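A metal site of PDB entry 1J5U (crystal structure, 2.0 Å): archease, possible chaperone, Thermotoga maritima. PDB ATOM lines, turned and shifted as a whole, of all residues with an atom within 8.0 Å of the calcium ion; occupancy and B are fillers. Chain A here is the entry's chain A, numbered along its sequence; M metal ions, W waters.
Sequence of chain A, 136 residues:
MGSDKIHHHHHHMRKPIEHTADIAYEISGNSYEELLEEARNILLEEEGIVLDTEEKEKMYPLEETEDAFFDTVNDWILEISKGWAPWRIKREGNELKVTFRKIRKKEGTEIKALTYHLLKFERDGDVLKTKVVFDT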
ATOM      1  N   ILE A  17     -19.031 -19.607 -24.896  1.00  0.00           N
ATOM      2  CA  ILE A  17     -18.940 -20.060 -23.511  1.00  0.00           C
ATOM      3  C   ILE A  17     -19.721 -19.067 -22.662  1.00  0.00           C
ATOM      4  O   ILE A  17     -19.669 -17.881 -22.921  1.00  0.00           O
ATOM      5  CB  ILE A  17     -17.465 -20.111 -22.991  1.00  0.00           C
ATOM      6  CG1 ILE A  17     -16.617 -19.016 -23.640  1.00  0.00           C
ATOM      7  CG2 ILE A  17     -16.834 -21.464 -23.288  1.00  0.00           C
ATOM      8  CD1 ILE A  17     -16.896 -17.624 -23.135  1.00  0.00           C
ATOM      9  N   GLU A  18     -20.473 -19.557 -21.694  1.00  0.00           N
ATOM     10  CA  GLU A  18     -21.225 -18.673 -20.804  1.00  0.00           C
ATOM     11  C   GLU A  18     -20.480 -18.643 -19.465  1.00  0.00           C
ATOM     12  O   GLU A  18     -19.992 -19.680 -18.989  1.00  0.00           O
ATOM     13  CB  GLU A  18     -22.640 -19.192 -20.579  1.00  0.00           C
ATOM     14  CG  GLU A  18     -23.528 -19.190 -21.811  1.00  0.00           C
ATOM     15  CD  GLU A  18     -24.916 -19.689 -21.484  1.00  0.00           C
ATOM     16  OE1 GLU A  18     -25.022 -20.773 -20.871  1.00  0.00           O
ATOM     17  OE2 GLU A  18     -25.910 -19.011 -21.850  1.00  0.00           O
ATOM     18  N   HIS A  19     -20.377 -17.473 -18.857  1.00  0.00           N
ATOM     19  CA  HIS A  19     -19.703 -17.353 -17.560  1.00  0.00           C
ATOM     20  C   HIS A  19     -20.575 -16.502 -16.639  1.00  0.00           C
ATOM     21  O   HIS A  19     -21.346 -15.706 -17.131  1.00  0.00           O
ATOM     22  CB  HIS A  19     -18.373 -16.611 -17.690  1.00  0.00           C
ATOM     23  CG  HIS A  19     -17.344 -17.318 -18.516  1.00  0.00           C
ATOM     24  ND1 HIS A  19     -16.615 -18.435 -18.270  1.00  0.00           N
ATOM     25  CD2 HIS A  19     -16.861 -16.806 -19.702  1.00  0.00           C
ATOM     26  CE1 HIS A  19     -15.709 -18.565 -19.294  1.00  0.00           C
ATOM     27  NE2 HIS A  19     -15.879 -17.572 -20.145  1.00  0.00           N
ATOM     28  N   THR A  20     -20.481 -16.668 -15.335  1.00  0.00           N
ATOM     29  CA  THR A  20     -21.221 -15.754 -14.464  1.00  0.00           C
ATOM     30  C   THR A  20     -20.134 -14.788 -13.979  1.00  0.00           C
ATOM     31  O   THR A  20     -20.422 -13.703 -13.469  1.00  0.00           O
ATOM     32  CB  THR A  20     -21.911 -16.464 -13.281  1.00  0.00           C
ATOM     33  OG1 THR A  20     -21.030 -17.438 -12.716  1.00  0.00           O
ATOM     34  CG2 THR A  20     -23.215 -17.139 -13.741  1.00  0.00           C
ATOM     35  N   ALA A  21     -18.880 -15.186 -14.171  1.00  0.00           N
ATOM     36  CA  ALA A  21     -17.754 -14.313 -13.809  1.00  0.00           C
ATOM     37  C   ALA A  21     -17.294 -13.614 -15.073  1.00  0.00           C
ATOM     38  O   ALA A  21     -16.385 -14.079 -15.780  1.00  0.00           O
ATOM     39  CB  ALA A  21     -16.612 -15.135 -13.177  1.00  0.00           C
ATOM     40  N   ASP A  22     -17.909 -12.485 -15.388  1.00  0.00           N
ATOM     41  CA  ASP A  22     -17.540 -11.742 -16.595  1.00  0.00           C
ATOM     42  C   ASP A  22     -16.604 -10.571 -16.430  1.00  0.00           C
ATOM     43  O   ASP A  22     -15.665 -10.414 -17.213  1.00  0.00           O
ATOM     44  CB  ASP A  22     -18.783 -11.277 -17.340  1.00  0.00           C
ATOM     45  CG  ASP A  22     -19.549 -12.430 -17.959  1.00  0.00           C
ATOM     46  OD1 ASP A  22     -18.965 -13.177 -18.766  1.00  0.00           O
ATOM     47  OD2 ASP A  22     -20.727 -12.600 -17.613  1.00  0.00           O
ATOM     48  N   ILE A  23     -16.855  -9.696 -15.459  1.00  0.00           N
ATOM     49  CA  ILE A  23     -15.972  -8.567 -15.243  1.00  0.00           C
ATOM     50  C   ILE A  23     -15.657  -8.483 -13.773  1.00  0.00           C
ATOM     51  O   ILE A  23     -16.502  -8.824 -12.926  1.00  0.00           O
ATOM     52  CB  ILE A  23     -16.582  -7.217 -15.740  1.00  0.00           C
ATOM     53  CG1 ILE A  23     -17.786  -6.822 -14.899  1.00  0.00           C
ATOM     54  CG2 ILE A  23     -16.988  -7.323 -17.209  1.00  0.00           C
ATOM     55  CD1 ILE A  23     -18.335  -5.434 -15.298  1.00  0.00           C
ATOM     56  N   LYS A 112     -25.829  -7.758 -15.193  1.00  0.00           N
ATOM     57  CA  LYS A 112     -26.923  -8.619 -14.774  1.00  0.00           C
ATOM     58  C   LYS A 112     -26.980  -8.880 -13.274  1.00  0.00           C
ATOM     59  O   LYS A 112     -28.052  -9.042 -12.689  1.00  0.00           O
ATOM     60  CB  LYS A 112     -26.830  -9.976 -15.478  1.00  0.00           C
ATOM     61  CG  LYS A 112     -26.994  -9.928 -16.989  1.00  0.00           C
ATOM     62  CD  LYS A 112     -26.877 -11.333 -17.565  1.00  0.00           C
ATOM     63  CE  LYS A 112     -26.897 -11.317 -19.086  1.00  0.00           C
ATOM     64  NZ  LYS A 112     -26.503 -12.658 -19.626  1.00  0.00           N
ATOM     65  N   THR A 115     -22.043 -11.316  -8.405  1.00  0.00           N
ATOM     66  CA  THR A 115     -21.983 -12.727  -8.006  1.00  0.00           C
ATOM     67  C   THR A 115     -21.271 -12.854  -6.676  1.00  0.00           C
ATOM     68  O   THR A 115     -20.769 -11.863  -6.114  1.00  0.00           O
ATOM     69  CB  THR A 115     -21.184 -13.569  -9.035  1.00  0.00           C
ATOM     70  OG1 THR A 115     -19.793 -13.204  -8.952  1.00  0.00           O
ATOM     71  CG2 THR A 115     -21.689 -13.317 -10.452  1.00  0.00           C
ATOM     72  N   PHE A 134     -18.871  -9.434 -11.487  1.00  0.00           N
ATOM     73  CA  PHE A 134     -20.196  -9.283 -12.047  1.00  0.00           C
ATOM     74  C   PHE A 134     -20.439 -10.156 -13.265  1.00  0.00           C
ATOM     75  O   PHE A 134     -19.512 -10.519 -14.004  1.00  0.00           O
ATOM     76  CB  PHE A 134     -20.457  -7.826 -12.452  1.00  0.00           C
ATOM     77  CG  PHE A 134     -20.329  -6.856 -11.330  1.00  0.00           C
ATOM     78  CD1 PHE A 134     -19.077  -6.361 -10.952  1.00  0.00           C
ATOM     79  CD2 PHE A 134     -21.466  -6.418 -10.640  1.00  0.00           C
ATOM     80  CE1 PHE A 134     -18.951  -5.442  -9.912  1.00  0.00           C
ATOM     81  CE2 PHE A 134     -21.356  -5.492  -9.600  1.00  0.00           C
ATOM     82  CZ  PHE A 134     -20.107  -5.001  -9.235  1.00  0.00           C
ATOM     83  N   ASP A 135     -21.716 -10.463 -13.445  1.00  0.00           N
ATOM     84  CA  ASP A 135     -22.200 -11.270 -14.540  1.00  0.00           C
ATOM     85  C   ASP A 135     -22.799 -10.295 -15.567  1.00  0.00           C
ATOM     86  O   ASP A 135     -23.533  -9.384 -15.210  1.00  0.00           O
ATOM     87  CB  ASP A 135     -23.264 -12.238 -13.984  1.00  0.00           C
ATOM     88  CG  ASP A 135     -23.877 -13.112 -15.052  1.00  0.00           C
ATOM     89  OD1 ASP A 135     -23.176 -13.396 -16.033  1.00  0.00           O
ATOM     90  OD2 ASP A 135     -25.048 -13.521 -14.924  1.00  0.00           O
ATOM     91  N   THR A 136     -22.442 -10.458 -16.847  1.00  0.00           N
ATOM     92  CA  THR A 136     -22.994  -9.603 -17.895  1.00  0.00           C
ATOM     93  C   THR A 136     -23.636 -10.485 -18.969  1.00  0.00           C
ATOM     94  O   THR A 136     -24.209  -9.932 -19.936  1.00  0.00           O
ATOM     95  CB  THR A 136     -21.916  -8.714 -18.579  1.00  0.00           C
ATOM     96  OG1 THR A 136     -20.911  -9.532 -19.183  1.00  0.00           O
ATOM     97  CG2 THR A 136     -21.237  -7.800 -17.543  1.00  0.00           C
ATOM     98  OXT THR A 136     -23.585 -11.706 -18.831  1.00  0.00           O
HETATM   99 CA    CA M   1     -22.648 -13.983 -18.299  1.00  0.00          CA
HETATM  100  O   HOH W   1     -25.314 -15.403 -17.130  1.00  0.00           O
HETATM  101  O   HOH W   2     -23.648 -13.793 -20.995  1.00  0.00           O
HETATM  102  O   HOH W   3     -23.690 -16.516 -18.854  1.00  0.00           O
HETATM  103  O   HOH W   4     -20.674 -14.532 -20.132  1.00  0.00           O
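The nearest printed residue that does not touch the calcium ion is Lys 112 (4.3 Å).
The calcium ion is bound by OD1 of Asp 135, O of His 19, OD2 of Asp 22, OXT of Thr 136, water W4, water W3 and water W2. The calcium ion has seven donor atoms within binding distance.
O of Thr 136 is in salt-bridge range of NZ of Lys 112 (3.6 Å). O of Phe 134 lies within hydrogen-bond range of N of Asp 22 (2.9 Å). The backbone carbonyl oxygen of Asp 135 sits at hydrogen-bond distance from the backbone NH of Lys 112 (2.8 Å). N of Asp 135 lies close to O of Thr 20 (3.5 Å).
Water W4 lies within hydrogen-bond range of the side-chain carboxylate of Asp 22 and the backbone NH of His 19.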
